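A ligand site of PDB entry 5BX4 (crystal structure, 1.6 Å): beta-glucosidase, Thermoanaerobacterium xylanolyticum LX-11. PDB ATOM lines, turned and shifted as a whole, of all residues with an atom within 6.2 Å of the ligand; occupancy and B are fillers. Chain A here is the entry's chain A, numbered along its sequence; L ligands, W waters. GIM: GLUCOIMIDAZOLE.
An oxygen (O6) of the ligand is in hydrogen-bond range of the side-chain carboxylate of Glu 762, at 2.6 Å.
NH1 of Arg 771 lies within hydrogen-bond range of O6 of the ligand.
An oxygen (O4) of the ligand lies within hydrogen-bond range of the guanidinium group (NH2) of Arg 777 (3.0 Å).
An oxygen (O3) of the ligand lies within hydrogen-bond range of a ring nitrogen (NE2) of His 492.
The backbone carbonyl oxygen (O) of Thr 576 sits at hydrogen-bond distance from an oxygen (O4) of the ligand (2.6 Å).
The side-chain carboxylate of Asp 437 lies within hydrogen-bond range of an oxygen (O3) of the ligand (2.5 Å).
O4 of the ligand is in hydrogen-bond range of OG1 of Thr 576, at 2.8 Å.
The side-chain carboxylate of Glu 426 is in hydrogen-bond range of an oxygen (O2) of the ligand (2.7 Å).
Tyr 430 touches the ligand.
Tyr 432 touches the ligand (CD2 to O2, 3.8 Å).
CG2 of Thr 435 touches O3 of the ligand, 3.7 Å away.
Tyr 508 touches the ligand (CD1 to O2, 3.4 Å).
Trp 516 touches the ligand.
Asp 578 touches the ligand (OD2 to C1, 3.5 Å).
Gln 712 touches the ligand.
Trp 717 touches the ligand (CH2 to C6, 3.7 Å).
OH of Tyr 775 touches C5 of the ligand (3.5 Å).
Hydrophobic or aromatic side chains within 4 Å of the ligand: Tyr 430, Tyr 432, His 492, Tyr 508, Trp 516 and Trp 717.
The nearest printed residue that does not touch the ligand is Val 438 (4.03 Å).
The backbone NH of Glu 426 lies within hydrogen-bond range of the backbone carbonyl oxygen of Tyr 432, at 2.8 Å.
N of Glu 762 lies within hydrogen-bond range of O of Arg 771, at 3.3 Å.
The guanidinium group of Arg 771 is in salt-bridge range of the side-chain carboxylate of Glu 715 (2.8 Å).
The guanidinium group of Arg 771 is in hydrogen-bond range of the side-chain hydroxyl of Tyr 430, 3.1 Å away.
OG1 of Thr 435 is in hydrogen-bond range of OE1 of Glu 426 (2.8 Å).
The backbone carbonyl oxygen of Tyr 577 lies close to the side-chain amide oxygen of Gln 712 (3.3 Å).
N of Tyr 508 sits at hydrogen-bond distance from OD2 of Asp 493, at 3.0 Å.
OE2 of Glu 426 sits at hydrogen-bond distance from OH of Tyr 775, at 2.6 Å.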
ATOM      1  N   GLU A 426      14.212 -15.667 -24.021  1.00  0.00           N
ATOM      2  CA  GLU A 426      12.889 -15.059 -24.129  1.00  0.00           C
ATOM      3  C   GLU A 426      11.840 -16.039 -23.624  1.00  0.00           C
ATOM      4  O   GLU A 426      11.002 -15.700 -22.808  1.00  0.00           O
ATOM      5  CB  GLU A 426      12.624 -14.664 -25.578  1.00  0.00           C
ATOM      6  CG  GLU A 426      11.245 -14.074 -25.836  1.00  0.00           C
ATOM      7  CD  GLU A 426      10.977 -13.764 -27.290  1.00  0.00           C
ATOM      8  OE1 GLU A 426      11.946 -13.564 -28.052  1.00  0.00           O
ATOM      9  OE2 GLU A 426       9.785 -13.670 -27.672  1.00  0.00           O
ATOM     10  N   TYR A 430      10.041 -19.621 -28.380  1.00  0.00           N
ATOM     11  CA  TYR A 430      10.788 -18.649 -29.164  1.00  0.00           C
ATOM     12  C   TYR A 430      12.163 -18.586 -28.521  1.00  0.00           C
ATOM     13  O   TYR A 430      12.428 -17.769 -27.638  1.00  0.00           O
ATOM     14  CB  TYR A 430      10.122 -17.284 -29.142  1.00  0.00           C
ATOM     15  CG  TYR A 430       8.618 -17.271 -29.193  1.00  0.00           C
ATOM     16  CD1 TYR A 430       7.909 -18.034 -30.114  1.00  0.00           C
ATOM     17  CD2 TYR A 430       7.877 -16.460 -28.336  1.00  0.00           C
ATOM     18  CE1 TYR A 430       6.529 -18.004 -30.166  1.00  0.00           C
ATOM     19  CE2 TYR A 430       6.493 -16.417 -28.383  1.00  0.00           C
ATOM     20  CZ  TYR A 430       5.825 -17.192 -29.306  1.00  0.00           C
ATOM     21  OH  TYR A 430       4.440 -17.127 -29.350  1.00  0.00           O
ATOM     22  N   TYR A 432      15.290 -17.625 -28.141  1.00  0.00           N
ATOM     23  CA  TYR A 432      16.216 -16.522 -28.404  1.00  0.00           C
ATOM     24  C   TYR A 432      16.771 -15.987 -27.089  1.00  0.00           C
ATOM     25  O   TYR A 432      16.000 -15.715 -26.158  1.00  0.00           O
ATOM     26  CB  TYR A 432      15.493 -15.409 -29.145  1.00  0.00           C
ATOM     27  CG  TYR A 432      14.762 -15.904 -30.363  1.00  0.00           C
ATOM     28  CD1 TYR A 432      15.451 -16.600 -31.346  1.00  0.00           C
ATOM     29  CD2 TYR A 432      13.401 -15.691 -30.526  1.00  0.00           C
ATOM     30  CE1 TYR A 432      14.789 -17.073 -32.474  1.00  0.00           C
ATOM     31  CE2 TYR A 432      12.740 -16.164 -31.654  1.00  0.00           C
ATOM     32  CZ  TYR A 432      13.447 -16.850 -32.612  1.00  0.00           C
ATOM     33  OH  TYR A 432      12.805 -17.329 -33.748  1.00  0.00           O
ATOM     34  N   THR A 435      16.393 -11.417 -25.768  1.00  0.00           N
ATOM     35  CA  THR A 435      15.595 -10.609 -26.680  1.00  0.00           C
ATOM     36  C   THR A 435      15.412  -9.218 -26.082  1.00  0.00           C
ATOM     37  O   THR A 435      14.772  -9.065 -25.039  1.00  0.00           O
ATOM     38  CB  THR A 435      14.237 -11.243 -26.958  1.00  0.00           C
ATOM     39  OG1 THR A 435      14.447 -12.515 -27.560  1.00  0.00           O
ATOM     40  CG2 THR A 435      13.388 -10.352 -27.895  1.00  0.00           C
ATOM     41  N   ASP A 437      13.945  -6.300 -26.836  1.00  0.00           N
ATOM     42  CA  ASP A 437      12.658  -5.623 -26.736  1.00  0.00           C
ATOM     43  C   ASP A 437      11.829  -6.180 -25.592  1.00  0.00           C
ATOM     44  O   ASP A 437      10.924  -5.492 -25.106  1.00  0.00           O
ATOM     45  CB  ASP A 437      11.866  -5.709 -28.058  1.00  0.00           C
ATOM     46  CG  ASP A 437      11.800  -7.101 -28.601  1.00  0.00           C
ATOM     47  OD1 ASP A 437      12.839  -7.585 -29.097  1.00  0.00           O
ATOM     48  OD2 ASP A 437      10.727  -7.724 -28.520  1.00  0.00           O
ATOM     49  N   VAL A 438      12.136  -7.423 -25.196  1.00  0.00           N
ATOM     50  CA  VAL A 438      11.509  -8.116 -24.067  1.00  0.00           C
ATOM     51  C   VAL A 438      12.273  -7.847 -22.771  1.00  0.00           C
ATOM     52  O   VAL A 438      11.636  -7.637 -21.711  1.00  0.00           O
ATOM     53  CB  VAL A 438      11.476  -9.637 -24.341  1.00  0.00           C
ATOM     54  CG1 VAL A 438      10.956 -10.406 -23.128  1.00  0.00           C
ATOM     55  CG2 VAL A 438      10.627  -9.931 -25.572  1.00  0.00           C
ATOM     56  N   HIS A 492      18.102  -7.809 -32.237  1.00  0.00           N
ATOM     57  CA  HIS A 492      16.944  -8.338 -31.521  1.00  0.00           C
ATOM     58  C   HIS A 492      17.341  -9.288 -30.381  1.00  0.00           C
ATOM     59  O   HIS A 492      16.700  -9.268 -29.319  1.00  0.00           O
ATOM     60  CB  HIS A 492      16.079  -9.096 -32.521  1.00  0.00           C
ATOM     61  CG  HIS A 492      14.873  -9.745 -31.928  1.00  0.00           C
ATOM     62  ND1 HIS A 492      14.868 -11.070 -31.534  1.00  0.00           N
ATOM     63  CD2 HIS A 492      13.640  -9.285 -31.683  1.00  0.00           C
ATOM     64  CE1 HIS A 492      13.682 -11.382 -31.068  1.00  0.00           C
ATOM     65  NE2 HIS A 492      12.901 -10.317 -31.156  1.00  0.00           N
ATOM     66  N   ASP A 493      18.338 -10.127 -30.621  1.00  0.00           N
ATOM     67  CA  ASP A 493      18.699 -11.190 -29.694  1.00  0.00           C
ATOM     68  C   ASP A 493      20.143 -11.617 -29.903  1.00  0.00           C
ATOM     69  O   ASP A 493      20.776 -11.248 -30.903  1.00  0.00           O
ATOM     70  CB  ASP A 493      17.745 -12.372 -29.862  1.00  0.00           C
ATOM     71  CG  ASP A 493      17.860 -13.004 -31.234  1.00  0.00           C
ATOM     72  OD1 ASP A 493      18.885 -13.670 -31.475  1.00  0.00           O
ATOM     73  OD2 ASP A 493      16.912 -12.820 -32.035  1.00  0.00           O
ATOM     74  N   TYR A 508      16.175 -14.559 -34.426  1.00  0.00           N
ATOM     75  CA  TYR A 508      14.798 -14.224 -34.771  1.00  0.00           C
ATOM     76  C   TYR A 508      14.654 -13.792 -36.233  1.00  0.00           C
ATOM     77  O   TYR A 508      15.461 -13.012 -36.709  1.00  0.00           O
ATOM     78  CB  TYR A 508      14.331 -13.089 -33.876  1.00  0.00           C
ATOM     79  CG  TYR A 508      12.983 -12.491 -34.153  1.00  0.00           C
ATOM     80  CD1 TYR A 508      11.817 -13.086 -33.691  1.00  0.00           C
ATOM     81  CD2 TYR A 508      12.872 -11.287 -34.851  1.00  0.00           C
ATOM     82  CE1 TYR A 508      10.571 -12.520 -33.936  1.00  0.00           C
ATOM     83  CE2 TYR A 508      11.644 -10.714 -35.085  1.00  0.00           C
ATOM     84  CZ  TYR A 508      10.508 -11.329 -34.629  1.00  0.00           C
ATOM     85  OH  TYR A 508       9.310 -10.725 -34.879  1.00  0.00           O
ATOM     86  N   TRP A 510      11.007 -13.664 -37.811  1.00  0.00           N
ATOM     87  CA  TRP A 510       9.616 -13.419 -38.195  1.00  0.00           C
ATOM     88  C   TRP A 510       9.463 -12.018 -38.826  1.00  0.00           C
ATOM     89  O   TRP A 510       8.704 -11.842 -39.798  1.00  0.00           O
ATOM     90  CB  TRP A 510       8.666 -13.567 -36.996  1.00  0.00           C
ATOM     91  CG  TRP A 510       7.267 -13.227 -37.347  1.00  0.00           C
ATOM     92  CD1 TRP A 510       6.555 -12.125 -36.949  1.00  0.00           C
ATOM     93  CD2 TRP A 510       6.397 -13.972 -38.204  1.00  0.00           C
ATOM     94  NE1 TRP A 510       5.297 -12.156 -37.495  1.00  0.00           N
ATOM     95  CE2 TRP A 510       5.169 -13.273 -38.260  1.00  0.00           C
ATOM     96  CE3 TRP A 510       6.523 -15.163 -38.930  1.00  0.00           C
ATOM     97  CZ2 TRP A 510       4.086 -13.732 -39.014  1.00  0.00           C
ATOM     98  CZ3 TRP A 510       5.440 -15.619 -39.671  1.00  0.00           C
ATOM     99  CH2 TRP A 510       4.243 -14.894 -39.713  1.00  0.00           C
ATOM    100  N   TRP A 516      13.516  -2.313 -36.798  1.00  0.00           N
ATOM    101  CA  TRP A 516      12.637  -2.036 -35.654  1.00  0.00           C
ATOM    102  C   TRP A 516      12.875  -0.642 -35.078  1.00  0.00           C
ATOM    103  O   TRP A 516      13.985  -0.120 -35.136  1.00  0.00           O
ATOM    104  CB  TRP A 516      12.767  -3.129 -34.588  1.00  0.00           C
ATOM    105  CG  TRP A 516      11.959  -4.341 -34.939  1.00  0.00           C
ATOM    106  CD1 TRP A 516      11.501  -4.706 -36.182  1.00  0.00           C
ATOM    107  CD2 TRP A 516      11.513  -5.385 -34.049  1.00  0.00           C
ATOM    108  NE1 TRP A 516      10.804  -5.878 -36.124  1.00  0.00           N
ATOM    109  CE2 TRP A 516      10.792  -6.312 -34.820  1.00  0.00           C
ATOM    110  CE3 TRP A 516      11.644  -5.598 -32.672  1.00  0.00           C
ATOM    111  CZ2 TRP A 516      10.206  -7.456 -34.265  1.00  0.00           C
ATOM    112  CZ3 TRP A 516      11.069  -6.727 -32.129  1.00  0.00           C
ATOM    113  CH2 TRP A 516      10.359  -7.639 -32.911  1.00  0.00           C
ATOM    114  N   GLN A 575       8.426  -3.543 -34.220  1.00  0.00           N
ATOM    115  CA  GLN A 575       8.697  -3.390 -32.786  1.00  0.00           C
ATOM    116  C   GLN A 575       8.145  -4.619 -32.051  1.00  0.00           C
ATOM    117  O   GLN A 575       7.603  -5.540 -32.660  1.00  0.00           O
ATOM    118  CB  GLN A 575       8.152  -2.067 -32.239  1.00  0.00           C
ATOM    119  CG  GLN A 575       6.825  -1.599 -32.825  1.00  0.00           C
ATOM    120  CD  GLN A 575       5.698  -2.577 -32.596  1.00  0.00           C
ATOM    121  OE1 GLN A 575       5.506  -3.046 -31.483  1.00  0.00           O
ATOM    122  NE2 GLN A 575       4.908  -2.851 -33.619  1.00  0.00           N
ATOM    123  N   THR A 576       8.300  -4.618 -30.726  1.00  0.00           N
ATOM    124  CA  THR A 576       7.988  -5.798 -29.895  1.00  0.00           C
ATOM    125  C   THR A 576       6.622  -6.446 -30.105  1.00  0.00           C
ATOM    126  O   THR A 576       6.486  -7.656 -29.931  1.00  0.00           O
ATOM    127  CB  THR A 576       8.184  -5.458 -28.389  1.00  0.00           C
ATOM    128  OG1 THR A 576       8.412  -6.651 -27.640  1.00  0.00           O
ATOM    129  CG2 THR A 576       7.017  -4.699 -27.826  1.00  0.00           C
ATOM    130  N   TYR A 577       5.616  -5.652 -30.449  1.00  0.00           N
ATOM    131  CA  TYR A 577       4.303  -6.198 -30.800  1.00  0.00           C
ATOM    132  C   TYR A 577       4.410  -6.615 -32.264  1.00  0.00           C
ATOM    133  O   TYR A 577       3.979  -5.891 -33.175  1.00  0.00           O
ATOM    134  CB  TYR A 577       3.182  -5.184 -30.553  1.00  0.00           C
ATOM    135  CG  TYR A 577       3.074  -4.716 -29.098  1.00  0.00           C
ATOM    136  CD1 TYR A 577       3.847  -3.667 -28.618  1.00  0.00           C
ATOM    137  CD2 TYR A 577       2.185  -5.336 -28.210  1.00  0.00           C
ATOM    138  CE1 TYR A 577       3.742  -3.221 -27.304  1.00  0.00           C
ATOM    139  CE2 TYR A 577       2.063  -4.895 -26.894  1.00  0.00           C
ATOM    140  CZ  TYR A 577       2.853  -3.859 -26.449  1.00  0.00           C
ATOM    141  OH  TYR A 577       2.744  -3.425 -25.147  1.00  0.00           O
ATOM    142  N   ASP A 578       5.007  -7.789 -32.462  1.00  0.00           N
ATOM    143  CA  ASP A 578       5.551  -8.177 -33.767  1.00  0.00           C
ATOM    144  C   ASP A 578       4.530  -8.738 -34.754  1.00  0.00           C
ATOM    145  O   ASP A 578       4.905  -9.207 -35.830  1.00  0.00           O
ATOM    146  CB  ASP A 578       6.755  -9.121 -33.602  1.00  0.00           C
ATOM    147  CG  ASP A 578       6.378 -10.537 -33.188  1.00  0.00           C
ATOM    148  OD1 ASP A 578       5.255 -10.765 -32.695  1.00  0.00           O
ATOM    149  OD2 ASP A 578       7.236 -11.433 -33.338  1.00  0.00           O
ATOM    150  N   GLN A 712      -2.676  -9.550 -31.071  1.00  0.00           N
ATOM    151  CA  GLN A 712      -1.926  -8.927 -29.967  1.00  0.00           C
ATOM    152  C   GLN A 712      -2.696  -7.809 -29.291  1.00  0.00           C
ATOM    153  O   GLN A 712      -2.567  -7.603 -28.085  1.00  0.00           O
ATOM    154  CB  GLN A 712      -0.552  -8.450 -30.449  1.00  0.00           C
ATOM    155  CG  GLN A 712       0.365  -9.617 -30.783  1.00  0.00           C
ATOM    156  CD  GLN A 712       1.732  -9.208 -31.294  1.00  0.00           C
ATOM    157  OE1 GLN A 712       1.931  -8.068 -31.743  1.00  0.00           O
ATOM    158  NE2 GLN A 712       2.682 -10.124 -31.232  1.00  0.00           N
ATOM    159  N   GLU A 715      -4.853  -9.367 -26.631  1.00  0.00           N
ATOM    160  CA  GLU A 715      -4.106 -10.067 -25.591  1.00  0.00           C
ATOM    161  C   GLU A 715      -3.805  -9.120 -24.418  1.00  0.00           C
ATOM    162  O   GLU A 715      -3.585  -7.925 -24.598  1.00  0.00           O
ATOM    163  CB  GLU A 715      -2.793 -10.633 -26.150  1.00  0.00           C
ATOM    164  CG  GLU A 715      -2.953 -11.839 -27.068  1.00  0.00           C
ATOM    165  CD  GLU A 715      -1.638 -12.380 -27.610  1.00  0.00           C
ATOM    166  OE1 GLU A 715      -0.698 -11.587 -27.813  1.00  0.00           O
ATOM    167  OE2 GLU A 715      -1.550 -13.596 -27.841  1.00  0.00           O
ATOM    168  N   TRP A 717      -0.738  -8.813 -22.034  1.00  0.00           N
ATOM    169  CA  TRP A 717       0.655  -9.218 -21.879  1.00  0.00           C
ATOM    170  C   TRP A 717       1.020  -9.049 -20.400  1.00  0.00           C
ATOM    171  O   TRP A 717       0.937  -7.964 -19.853  1.00  0.00           O
ATOM    172  CB  TRP A 717       1.569  -8.409 -22.793  1.00  0.00           C
ATOM    173  CG  TRP A 717       1.507  -8.850 -24.249  1.00  0.00           C
ATOM    174  CD1 TRP A 717       0.531  -9.621 -24.837  1.00  0.00           C
ATOM    175  CD2 TRP A 717       2.452  -8.544 -25.276  1.00  0.00           C
ATOM    176  NE1 TRP A 717       0.817  -9.802 -26.163  1.00  0.00           N
ATOM    177  CE2 TRP A 717       1.984  -9.151 -26.470  1.00  0.00           C
ATOM    178  CE3 TRP A 717       3.629  -7.802 -25.312  1.00  0.00           C
ATOM    179  CZ2 TRP A 717       2.676  -9.050 -27.684  1.00  0.00           C
ATOM    180  CZ3 TRP A 717       4.333  -7.712 -26.511  1.00  0.00           C
ATOM    181  CH2 TRP A 717       3.840  -8.330 -27.693  1.00  0.00           C
ATOM    182  N   GLU A 762       3.665 -15.200 -21.850  1.00  0.00           N
ATOM    183  CA  GLU A 762       3.600 -13.856 -22.436  1.00  0.00           C
ATOM    184  C   GLU A 762       2.195 -13.287 -22.303  1.00  0.00           C
ATOM    185  O   GLU A 762       1.991 -12.178 -21.799  1.00  0.00           O
ATOM    186  CB  GLU A 762       3.991 -13.910 -23.914  1.00  0.00           C
ATOM    187  CG  GLU A 762       3.646 -12.680 -24.738  1.00  0.00           C
ATOM    188  CD  GLU A 762       4.708 -11.590 -24.701  1.00  0.00           C
ATOM    189  OE1 GLU A 762       4.908 -10.974 -23.612  1.00  0.00           O
ATOM    190  OE2 GLU A 762       5.338 -11.320 -25.768  1.00  0.00           O
ATOM    191  N   ARG A 771      -0.557 -17.749 -24.729  1.00  0.00           N
ATOM    192  CA  ARG A 771       0.508 -17.870 -25.706  1.00  0.00           C
ATOM    193  C   ARG A 771       1.857 -17.753 -24.998  1.00  0.00           C
ATOM    194  O   ARG A 771       2.104 -16.775 -24.275  1.00  0.00           O
ATOM    195  CB  ARG A 771       0.383 -16.805 -26.795  1.00  0.00           C
ATOM    196  CG  ARG A 771       1.423 -16.893 -27.892  1.00  0.00           C
ATOM    197  CD  ARG A 771       1.048 -16.010 -29.064  1.00  0.00           C
ATOM    198  NE  ARG A 771       0.998 -14.583 -28.704  1.00  0.00           N
ATOM    199  CZ  ARG A 771       2.055 -13.800 -28.570  1.00  0.00           C
ATOM    200  NH1 ARG A 771       3.278 -14.281 -28.730  1.00  0.00           N
ATOM    201  NH2 ARG A 771       1.893 -12.521 -28.249  1.00  0.00           N
ATOM    202  N   TYR A 775       7.806 -17.394 -19.848  1.00  0.00           N
ATOM    203  CA  TYR A 775       8.172 -16.190 -20.602  1.00  0.00           C
ATOM    204  C   TYR A 775       8.949 -15.186 -19.751  1.00  0.00           C
ATOM    205  O   TYR A 775       8.669 -15.010 -18.583  1.00  0.00           O
ATOM    206  CB  TYR A 775       6.912 -15.545 -21.216  1.00  0.00           C
ATOM    207  CG  TYR A 775       7.229 -14.757 -22.456  1.00  0.00           C
ATOM    208  CD1 TYR A 775       7.494 -15.406 -23.666  1.00  0.00           C
ATOM    209  CD2 TYR A 775       7.298 -13.377 -22.432  1.00  0.00           C
ATOM    210  CE1 TYR A 775       7.825 -14.692 -24.790  1.00  0.00           C
ATOM    211  CE2 TYR A 775       7.632 -12.653 -23.559  1.00  0.00           C
ATOM    212  CZ  TYR A 775       7.884 -13.324 -24.741  1.00  0.00           C
ATOM    213  OH  TYR A 775       8.211 -12.597 -25.861  1.00  0.00           O
ATOM    214  N   ARG A 777       9.182 -11.784 -19.992  1.00  0.00           N
ATOM    215  CA  ARG A 777       8.607 -10.441 -19.772  1.00  0.00           C
ATOM    216  C   ARG A 777       7.983 -10.190 -18.374  1.00  0.00           C
ATOM    217  O   ARG A 777       8.213  -9.118 -17.820  1.00  0.00           O
ATOM    218  CB  ARG A 777       7.609 -10.057 -20.876  1.00  0.00           C
ATOM    219  CG  ARG A 777       7.664  -8.568 -21.235  1.00  0.00           C
ATOM    220  CD  ARG A 777       6.613  -8.150 -22.260  1.00  0.00           C
ATOM    221  NE  ARG A 777       6.696  -8.878 -23.530  1.00  0.00           N
ATOM    222  CZ  ARG A 777       7.277  -8.439 -24.662  1.00  0.00           C
ATOM    223  NH1 ARG A 777       7.887  -7.265 -24.726  1.00  0.00           N
ATOM    224  NH2 ARG A 777       7.246  -9.209 -25.745  1.00  0.00           N
HETATM  225  C1  GIM L   1       8.661 -12.949 -30.539  1.00  0.00           C
HETATM  226  C2  GIM L   1       9.834 -12.045 -30.571  1.00  0.00           C
HETATM  227  N10 GIM L   1       7.527 -12.735 -29.900  1.00  0.00           N
HETATM  228  C3  GIM L   1       9.644 -10.889 -29.563  1.00  0.00           C
HETATM  229  C4  GIM L   1       8.185 -10.416 -29.500  1.00  0.00           C
HETATM  230  C5  GIM L   1       7.272 -11.552 -29.043  1.00  0.00           C
HETATM  231  C6  GIM L   1       5.805 -11.151 -29.023  1.00  0.00           C
HETATM  232  C7  GIM L   1       7.354 -14.612 -30.974  1.00  0.00           C
HETATM  233  C8  GIM L   1       6.684 -13.754 -30.148  1.00  0.00           C
HETATM  234  N1  GIM L   1       8.571 -14.106 -31.199  1.00  0.00           N
HETATM  235  O3  GIM L   1      10.436  -9.793 -29.978  1.00  0.00           O
HETATM  236  O2  GIM L   1      11.075 -12.738 -30.423  1.00  0.00           O
HETATM  237  O4  GIM L   1       8.052  -9.301 -28.606  1.00  0.00           O
HETATM  238  O6  GIM L   1       5.016 -12.044 -28.229  1.00  0.00           O
HETATM  239  O   HOH W   1       9.685 -15.845 -33.099  1.00  0.00           O
